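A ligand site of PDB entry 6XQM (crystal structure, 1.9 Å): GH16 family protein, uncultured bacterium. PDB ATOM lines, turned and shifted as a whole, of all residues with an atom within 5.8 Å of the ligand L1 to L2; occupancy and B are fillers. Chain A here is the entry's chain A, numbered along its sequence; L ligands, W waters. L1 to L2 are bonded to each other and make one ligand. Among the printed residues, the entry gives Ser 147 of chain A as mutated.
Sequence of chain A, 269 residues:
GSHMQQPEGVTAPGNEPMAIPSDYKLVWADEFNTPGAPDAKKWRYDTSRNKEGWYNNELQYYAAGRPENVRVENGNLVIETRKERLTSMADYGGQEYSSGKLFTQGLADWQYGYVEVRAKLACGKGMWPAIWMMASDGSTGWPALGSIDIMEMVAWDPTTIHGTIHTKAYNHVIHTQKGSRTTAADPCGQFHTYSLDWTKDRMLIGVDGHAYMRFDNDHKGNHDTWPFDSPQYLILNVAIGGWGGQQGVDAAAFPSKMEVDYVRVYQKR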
ATOM      1  N   TYR A  55      34.250  20.365 -32.093  1.00  0.00           N
ATOM      2  CA  TYR A  55      34.156  19.082 -32.815  1.00  0.00           C
ATOM      3  C   TYR A  55      32.778  19.000 -33.482  1.00  0.00           C
ATOM      4  O   TYR A  55      32.002  19.900 -33.317  1.00  0.00           O
ATOM      5  CB  TYR A  55      34.442  17.955 -31.805  1.00  0.00           C
ATOM      6  CG  TYR A  55      35.785  18.046 -31.116  1.00  0.00           C
ATOM      7  CD1 TYR A  55      36.952  17.787 -31.810  1.00  0.00           C
ATOM      8  CD2 TYR A  55      35.890  18.355 -29.773  1.00  0.00           C
ATOM      9  CE1 TYR A  55      38.203  17.837 -31.189  1.00  0.00           C
ATOM     10  CE2 TYR A  55      37.120  18.481 -29.148  1.00  0.00           C
ATOM     11  CZ  TYR A  55      38.275  18.182 -29.849  1.00  0.00           C
ATOM     12  OH  TYR A  55      39.484  18.310 -29.236  1.00  0.00           O
ATOM     13  N   ASN A  56      32.503  17.937 -34.237  1.00  0.00           N
ATOM     14  CA  ASN A  56      31.182  17.668 -34.863  1.00  0.00           C
ATOM     15  C   ASN A  56      30.759  18.789 -35.841  1.00  0.00           C
ATOM     16  O   ASN A  56      29.518  19.023 -35.987  1.00  0.00           O
ATOM     17  CB  ASN A  56      30.125  17.439 -33.791  1.00  0.00           C
ATOM     18  CG  ASN A  56      30.540  16.494 -32.684  1.00  0.00           C
ATOM     19  OD1 ASN A  56      30.871  15.329 -32.956  1.00  0.00           O
ATOM     20  ND2 ASN A  56      30.589  16.983 -31.466  1.00  0.00           N
ATOM     21  N   GLU A  58      30.631  21.790 -35.355  1.00  0.00           N
ATOM     22  CA  GLU A  58      29.847  22.750 -34.564  1.00  0.00           C
ATOM     23  C   GLU A  58      30.237  24.205 -34.918  1.00  0.00           C
ATOM     24  O   GLU A  58      31.386  24.492 -35.310  1.00  0.00           O
ATOM     25  CB  GLU A  58      30.030  22.485 -33.078  1.00  0.00           C
ATOM     26  CG  GLU A  58      29.255  21.283 -32.619  1.00  0.00           C
ATOM     27  CD  GLU A  58      29.647  20.771 -31.242  1.00  0.00           C
ATOM     28  OE1 GLU A  58      30.228  21.561 -30.464  1.00  0.00           O
ATOM     29  OE2 GLU A  58      29.374  19.581 -30.978  1.00  0.00           O
ATOM     30  N   LYS A 101      29.218  26.378 -22.382  1.00  0.00           N
ATOM     31  CA  LYS A 101      29.581  25.012 -21.976  1.00  0.00           C
ATOM     32  C   LYS A 101      30.183  25.092 -20.576  1.00  0.00           C
ATOM     33  O   LYS A 101      31.216  25.721 -20.431  1.00  0.00           O
ATOM     34  CB  LYS A 101      30.629  24.393 -22.914  1.00  0.00           C
ATOM     35  CG  LYS A 101      30.943  22.926 -22.616  1.00  0.00           C
ATOM     36  CD  LYS A 101      31.932  22.310 -23.549  1.00  0.00           C
ATOM     37  CE  LYS A 101      32.359  20.939 -23.106  1.00  0.00           C
ATOM     38  NZ  LYS A 101      33.383  20.473 -24.063  1.00  0.00           N
ATOM     39  N   TRP A 128      21.461  22.230 -30.311  1.00  0.00           N
ATOM     40  CA  TRP A 128      21.816  20.864 -29.882  1.00  0.00           C
ATOM     41  C   TRP A 128      22.153  20.894 -28.395  1.00  0.00           C
ATOM     42  O   TRP A 128      23.293  20.913 -28.023  1.00  0.00           O
ATOM     43  CB  TRP A 128      22.961  20.416 -30.768  1.00  0.00           C
ATOM     44  CG  TRP A 128      23.516  19.052 -30.475  1.00  0.00           C
ATOM     45  CD1 TRP A 128      23.070  18.103 -29.603  1.00  0.00           C
ATOM     46  CD2 TRP A 128      24.657  18.488 -31.114  1.00  0.00           C
ATOM     47  NE1 TRP A 128      23.855  16.968 -29.667  1.00  0.00           N
ATOM     48  CE2 TRP A 128      24.849  17.181 -30.589  1.00  0.00           C
ATOM     49  CE3 TRP A 128      25.551  18.966 -32.083  1.00  0.00           C
ATOM     50  CZ2 TRP A 128      25.934  16.391 -30.937  1.00  0.00           C
ATOM     51  CZ3 TRP A 128      26.585  18.167 -32.490  1.00  0.00           C
ATOM     52  CH2 TRP A 128      26.759  16.881 -31.932  1.00  0.00           C
ATOM     53  N   PRO A 129      21.157  21.039 -27.521  1.00  0.00           N
ATOM     54  CA  PRO A 129      21.380  21.033 -26.079  1.00  0.00           C
ATOM     55  C   PRO A 129      21.859  19.633 -25.674  1.00  0.00           C
ATOM     56  O   PRO A 129      21.383  18.613 -26.269  1.00  0.00           O
ATOM     57  CB  PRO A 129      20.000  21.372 -25.513  1.00  0.00           C
ATOM     58  CG  PRO A 129      19.047  20.868 -26.576  1.00  0.00           C
ATOM     59  CD  PRO A 129      19.733  21.112 -27.889  1.00  0.00           C
ATOM     60  N   ALA A 130      22.751  19.588 -24.675  1.00  0.00           N
ATOM     61  CA  ALA A 130      23.301  18.287 -24.150  1.00  0.00           C
ATOM     62  C   ALA A 130      23.530  18.353 -22.650  1.00  0.00           C
ATOM     63  O   ALA A 130      23.859  19.435 -22.145  1.00  0.00           O
ATOM     64  CB  ALA A 130      24.572  17.932 -24.874  1.00  0.00           C
ATOM     65  N   TRP A 132      25.651  15.646 -20.274  1.00  0.00           N
ATOM     66  CA  TRP A 132      26.531  14.475 -20.559  1.00  0.00           C
ATOM     67  C   TRP A 132      27.744  14.471 -19.639  1.00  0.00           C
ATOM     68  O   TRP A 132      27.985  15.405 -18.874  1.00  0.00           O
ATOM     69  CB  TRP A 132      26.920  14.392 -22.046  1.00  0.00           C
ATOM     70  CG  TRP A 132      27.726  15.508 -22.654  1.00  0.00           C
ATOM     71  CD1 TRP A 132      27.320  16.805 -22.753  1.00  0.00           C
ATOM     72  CD2 TRP A 132      28.980  15.428 -23.343  1.00  0.00           C
ATOM     73  NE1 TRP A 132      28.251  17.536 -23.424  1.00  0.00           N
ATOM     74  CE2 TRP A 132      29.282  16.731 -23.802  1.00  0.00           C
ATOM     75  CE3 TRP A 132      29.935  14.411 -23.559  1.00  0.00           C
ATOM     76  CZ2 TRP A 132      30.430  17.040 -24.520  1.00  0.00           C
ATOM     77  CZ3 TRP A 132      31.047  14.694 -24.316  1.00  0.00           C
ATOM     78  CH2 TRP A 132      31.333  15.996 -24.746  1.00  0.00           C
ATOM     79  N   MET A 133      28.463  13.387 -19.697  1.00  0.00           N
ATOM     80  CA  MET A 133      29.660  13.185 -18.841  1.00  0.00           C
ATOM     81  C   MET A 133      30.792  12.608 -19.688  1.00  0.00           C
ATOM     82  O   MET A 133      30.525  11.967 -20.774  1.00  0.00           O
ATOM     83  CB  MET A 133      29.329  12.210 -17.727  1.00  0.00           C
ATOM     84  CG  MET A 133      28.004  12.524 -17.088  1.00  0.00           C
ATOM     85  SD  MET A 133      27.678  11.450 -15.624  1.00  0.00           S
ATOM     86  CE  MET A 133      28.782  12.257 -14.455  1.00  0.00           C
ATOM     87  N   MET A 134      31.990  12.845 -19.206  1.00  0.00           N
ATOM     88  CA  MET A 134      33.236  12.296 -19.763  1.00  0.00           C
ATOM     89  C   MET A 134      34.115  11.790 -18.604  1.00  0.00           C
ATOM     90  O   MET A 134      34.038  12.380 -17.490  1.00  0.00           O
ATOM     91  CB  MET A 134      33.986  13.404 -20.487  1.00  0.00           C
ATOM     92  CG  MET A 134      33.384  13.769 -21.861  1.00  0.00           C
ATOM     93  SD  MET A 134      34.276  13.080 -23.294  1.00  0.00           S
ATOM     94  CE  MET A 134      35.936  13.748 -23.095  1.00  0.00           C
ATOM     95  N   TRP A 142      39.335  10.295 -26.538  1.00  0.00           N
ATOM     96  CA  TRP A 142      37.939  10.027 -26.975  1.00  0.00           C
ATOM     97  C   TRP A 142      38.045   9.224 -28.267  1.00  0.00           C
ATOM     98  O   TRP A 142      38.817   9.612 -29.132  1.00  0.00           O
ATOM     99  CB  TRP A 142      37.111  11.321 -27.145  1.00  0.00           C
ATOM    100  CG  TRP A 142      35.656  11.017 -27.342  1.00  0.00           C
ATOM    101  CD1 TRP A 142      34.678  10.946 -26.403  1.00  0.00           C
ATOM    102  CD2 TRP A 142      35.041  10.615 -28.571  1.00  0.00           C
ATOM    103  NE1 TRP A 142      33.499  10.526 -26.951  1.00  0.00           N
ATOM    104  CE2 TRP A 142      33.684  10.360 -28.290  1.00  0.00           C
ATOM    105  CE3 TRP A 142      35.501  10.475 -29.884  1.00  0.00           C
ATOM    106  CZ2 TRP A 142      32.798   9.936 -29.278  1.00  0.00           C
ATOM    107  CZ3 TRP A 142      34.627  10.090 -30.864  1.00  0.00           C
ATOM    108  CH2 TRP A 142      33.295   9.822 -30.552  1.00  0.00           C
ATOM    109  N   SER A 147      32.125   8.048 -22.535  1.00  0.00           N
ATOM    110  CA  SER A 147      31.297   9.269 -22.375  1.00  0.00           C
ATOM    111  C   SER A 147      29.835   8.846 -22.261  1.00  0.00           C
ATOM    112  O   SER A 147      29.450   7.748 -22.812  1.00  0.00           O
ATOM    113  CB  SER A 147      31.581  10.266 -23.463  1.00  0.00           C
ATOM    114  OG  SER A 147      30.989   9.891 -24.688  1.00  0.00           O
ATOM    115  N   ILE A 148      29.079   9.634 -21.518  1.00  0.00           N
ATOM    116  CA  ILE A 148      27.701   9.306 -21.109  1.00  0.00           C
ATOM    117  C   ILE A 148      26.784  10.474 -21.503  1.00  0.00           C
ATOM    118  O   ILE A 148      26.803  11.521 -20.797  1.00  0.00           O
ATOM    119  CB  ILE A 148      27.603   8.952 -19.621  1.00  0.00           C
ATOM    120  CG1 ILE A 148      28.667   7.921 -19.184  1.00  0.00           C
ATOM    121  CG2 ILE A 148      26.215   8.457 -19.349  1.00  0.00           C
ATOM    122  CD1 ILE A 148      28.725   7.693 -17.640  1.00  0.00           C
ATOM    123  N   ASP A 149      25.903  10.254 -22.491  1.00  0.00           N
ATOM    124  CA  ASP A 149      24.916  11.299 -22.869  1.00  0.00           C
ATOM    125  C   ASP A 149      23.611  11.039 -22.117  1.00  0.00           C
ATOM    126  O   ASP A 149      22.805  10.189 -22.616  1.00  0.00           O
ATOM    127  CB  ASP A 149      24.691  11.333 -24.394  1.00  0.00           C
ATOM    128  CG  ASP A 149      25.907  11.850 -25.146  1.00  0.00           C
ATOM    129  OD1 ASP A 149      26.081  13.128 -25.251  1.00  0.00           O
ATOM    130  OD2 ASP A 149      26.709  11.020 -25.572  1.00  0.00           O
ATOM    131  N   GLU A 152      20.543  14.127 -25.011  1.00  0.00           N
ATOM    132  CA  GLU A 152      20.742  15.035 -26.151  1.00  0.00           C
ATOM    133  C   GLU A 152      19.426  15.208 -26.885  1.00  0.00           C
ATOM    134  O   GLU A 152      18.587  14.241 -26.968  1.00  0.00           O
ATOM    135  CB  GLU A 152      21.801  14.559 -27.147  1.00  0.00           C
ATOM    136  CG  GLU A 152      23.209  14.463 -26.598  1.00  0.00           C
ATOM    137  CD  GLU A 152      24.166  13.746 -27.528  1.00  0.00           C
ATOM    138  OE1 GLU A 152      24.788  14.404 -28.425  1.00  0.00           O
ATOM    139  OE2 GLU A 152      24.195  12.496 -27.445  1.00  0.00           O
ATOM    140  N   HIS A 166      29.187   6.101 -25.361  1.00  0.00           N
ATOM    141  CA  HIS A 166      30.271   5.936 -26.342  1.00  0.00           C
ATOM    142  C   HIS A 166      31.450   5.257 -25.666  1.00  0.00           C
ATOM    143  O   HIS A 166      31.834   5.727 -24.575  1.00  0.00           O
ATOM    144  CB  HIS A 166      30.659   7.285 -26.913  1.00  0.00           C
ATOM    145  CG  HIS A 166      29.531   7.959 -27.604  1.00  0.00           C
ATOM    146  ND1 HIS A 166      29.270   7.771 -28.931  1.00  0.00           N
ATOM    147  CD2 HIS A 166      28.579   8.768 -27.133  1.00  0.00           C
ATOM    148  CE1 HIS A 166      28.183   8.486 -29.260  1.00  0.00           C
ATOM    149  NE2 HIS A 166      27.716   9.106 -28.168  1.00  0.00           N
ATOM    150  N   HIS A 172      29.925   6.898 -32.195  1.00  0.00           N
ATOM    151  CA  HIS A 172      29.163   7.443 -33.356  1.00  0.00           C
ATOM    152  C   HIS A 172      30.081   7.541 -34.582  1.00  0.00           C
ATOM    153  O   HIS A 172      29.564   7.417 -35.700  1.00  0.00           O
ATOM    154  CB  HIS A 172      28.485   8.783 -33.047  1.00  0.00           C
ATOM    155  CG  HIS A 172      29.470   9.883 -32.798  1.00  0.00           C
ATOM    156  ND1 HIS A 172      30.069  10.568 -33.825  1.00  0.00           N
ATOM    157  CD2 HIS A 172      29.909  10.423 -31.630  1.00  0.00           C
ATOM    158  CE1 HIS A 172      30.843  11.506 -33.334  1.00  0.00           C
ATOM    159  NE2 HIS A 172      30.803  11.407 -31.970  1.00  0.00           N
ATOM    160  N   VAL A 173      31.390   7.592 -34.419  1.00  0.00           N
ATOM    161  CA  VAL A 173      32.316   7.749 -35.569  1.00  0.00           C
ATOM    162  C   VAL A 173      32.237   6.514 -36.451  1.00  0.00           C
ATOM    163  O   VAL A 173      32.306   6.673 -37.691  1.00  0.00           O
ATOM    164  CB  VAL A 173      33.754   8.056 -35.134  1.00  0.00           C
ATOM    165  CG1 VAL A 173      34.677   8.055 -36.341  1.00  0.00           C
ATOM    166  CG2 VAL A 173      33.774   9.392 -34.366  1.00  0.00           C
ATOM    167  N   ASN A 237      25.725  21.987 -21.928  1.00  0.00           N
ATOM    168  CA  ASN A 237      26.109  22.871 -23.056  1.00  0.00           C
ATOM    169  C   ASN A 237      24.961  22.999 -24.049  1.00  0.00           C
ATOM    170  O   ASN A 237      24.104  22.119 -24.089  1.00  0.00           O
ATOM    171  CB  ASN A 237      27.368  22.402 -23.806  1.00  0.00           C
ATOM    172  CG  ASN A 237      27.145  21.093 -24.504  1.00  0.00           C
ATOM    173  OD1 ASN A 237      27.157  20.058 -23.843  1.00  0.00           O
ATOM    174  ND2 ASN A 237      26.870  21.144 -25.800  1.00  0.00           N
HETATM  175  C1  LIG L   1      28.493  12.766 -27.450  1.00  0.00           C
HETATM  176  C2  LIG L   1      29.404  13.014 -28.602  1.00  0.00           C
HETATM  177  C3  LIG L   1      30.188  14.349 -28.324  1.00  0.00           C
HETATM  178  C4  LIG L   1      29.230  15.592 -28.099  1.00  0.00           C
HETATM  179  C5  LIG L   1      28.337  15.242 -26.909  1.00  0.00           C
HETATM  180  C6  LIG L   1      27.267  16.307 -26.618  1.00  0.00           C
HETATM  181  O1  LIG L   1      29.393  12.337 -26.383  1.00  0.00           O
HETATM  182  O2  LIG L   1      30.279  11.903 -28.689  1.00  0.00           O
HETATM  183  O3  LIG L   1      31.060  14.622 -29.421  1.00  0.00           O
HETATM  184  O4  LIG L   1      29.997  16.870 -28.014  1.00  0.00           O
HETATM  185  O5  LIG L   1      27.674  13.985 -27.173  1.00  0.00           O
HETATM  186  O6  LIG L   1      26.227  16.419 -27.637  1.00  0.00           O
HETATM  187  C1  LG2 L   2      33.109  14.436 -30.719  1.00  0.00           C
HETATM  188  C2  LG2 L   2      34.605  14.107 -30.636  1.00  0.00           C
HETATM  189  C3  LG2 L   2      35.241  14.741 -29.380  1.00  0.00           C
HETATM  190  C4  LG2 L   2      34.456  14.393 -28.107  1.00  0.00           C
HETATM  191  C5  LG2 L   2      35.002  14.981 -26.814  1.00  0.00           C
HETATM  192  C6  LG2 L   2      32.413  14.258 -29.390  1.00  0.00           C
HETATM  193  O1  LG2 L   2      32.454  13.658 -31.755  1.00  0.00           O
HETATM  194  O2  LG2 L   2      35.311  14.408 -31.837  1.00  0.00           O
HETATM  195  O3  LG2 L   2      36.501  14.151 -29.198  1.00  0.00           O
HETATM  196  O4  LG2 L   2      33.139  14.824 -28.300  1.00  0.00           O
HETATM  197  O5  LG2 L   2      34.888  16.396 -26.965  1.00  0.00           O
HETATM  198  C1  LG3 L   3      24.742  10.112 -32.420  1.00  0.00           C
HETATM  199  C2  LG3 L   3      24.759   9.866 -30.887  1.00  0.00           C
HETATM  200  C3  LG3 L   3      25.138  11.125 -30.065  1.00  0.00           C
HETATM  201  C4  LG3 L   3      26.288  11.945 -30.670  1.00  0.00           C
HETATM  202  C5  LG3 L   3      25.929  12.366 -32.092  1.00  0.00           C
HETATM  203  C6  LG3 L   3      27.185  13.005 -32.709  1.00  0.00           C
HETATM  204  O1  LG3 L   3      23.685   9.746 -33.306  1.00  0.00           O
HETATM  205  O2  LG3 L   3      23.527   9.364 -30.345  1.00  0.00           O
HETATM  206  O3  LG3 L   3      25.466  10.829 -28.713  1.00  0.00           O
HETATM  207  O4  LG3 L   3      26.631  13.085 -29.874  1.00  0.00           O
HETATM  208  O5  LG3 L   3      25.641  11.149 -32.828  1.00  0.00           O
HETATM  209  O6  LG3 L   3      26.917  13.371 -34.066  1.00  0.00           O
HETATM  210  O   HOH W   1      36.289  17.781 -25.168  1.00  0.00           O
HETATM  211  O   HOH W   2      32.372  17.709 -27.955  1.00  0.00           O
HETATM  212  O   HOH W   3      28.649  18.926 -28.559  1.00  0.00           O
HETATM  213  O   HOH W   4      25.792  19.003 -27.742  1.00  0.00           O
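An oxygen (O6) of LIG L1 is in hydrogen-bond range of the side-chain carboxylate (OE1) of Glu 152, 2.6 Å away.
The side-chain amide oxygen (OD1) of Asn 56 lies within hydrogen-bond range of an oxygen (O1) of LG2 L2 (2.6 Å).
An oxygen (O6) of LIG L1 sits at hydrogen-bond distance from the indole nitrogen of Trp 128, at 3.2 Å.
OD2 of Asp 149 is in hydrogen-bond range of O1 of LIG L1.
A ring nitrogen (NE2) of His 166 lies within hydrogen-bond range of an oxygen (O3) of LG3 L3, 2.9 Å away.
The side-chain carboxylate (OE2) of Glu 152 lies within hydrogen-bond range of an oxygen (O3) of LG3 L3.
OG of Ser 147 lies within hydrogen-bond range of O1 of LIG L1 (3.4 Å).
An oxygen (O3) of LG3 L3 sits at hydrogen-bond distance from the side-chain carboxylate (OD2) of Asp 149.
An oxygen (O1) of LG2 L2 is in hydrogen-bond range of a ring nitrogen (NE2) of His 172 (2.8 Å).
O5 of LIG L1 lies within hydrogen-bond range of O4 of LG3 L3.
The side-chain carboxylate (OD2) of Asp 149 lies close to a ring nitrogen (NE2) of His 166.
The indole nitrogen (NE1) of Trp 142 lies within hydrogen-bond range of the side-chain hydroxyl (OG) of Ser 147, 3.4 Å away.
The backbone carbonyl oxygen (O) of Asn 237 is in hydrogen-bond range of the backbone NH (N) of Ala 130.
The side-chain amide nitrogen (ND2) of Asn 56 is in hydrogen-bond range of the side-chain carboxylate (OE2) of Glu 58, 2.9 Å away.
The indole nitrogen (NE1) of Trp 132 lies within hydrogen-bond range of the side-chain amide oxygen (OD1) of Asn 237 (2.8 Å).
The backbone NH (N) of His 166 sits at hydrogen-bond distance from the backbone carbonyl oxygen (O) of Ser 147 (3.0 Å).
The side-chain carboxylate (OE1) of Glu 152 is in hydrogen-bond range of the indole nitrogen (NE1) of Trp 128.
The backbone NH (N) of His 172 lies within hydrogen-bond range of a ring nitrogen (ND1) of His 166.
Merely in contact with the ligand L1 to L2: Tyr 55 (3.6 Å), Ala 130 (3.6 Å), Trp 132 (3.5 Å), Trp 142 (3.2 Å) and His 166 (3.7 Å).
Hydrophobic or aromatic side chains within 4 Å of the ligand L1 to L2: Tyr 55, Trp 128, Ala 130, Trp 132, Trp 142, His 166 and His 172.
The nearest printed residue that does not touch the ligand L1 to L2 is Met 134 (4.03 Å).
Water W3 bridges an oxygen (O4) of LIG L1 (2.5 Å) and the side-chain carboxylate (OE2) of Glu 58 (2.6 Å).
Water W4 lies within hydrogen-bond range of O6 of LIG L1, ND2 of Asn 237 and O of Trp 128.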
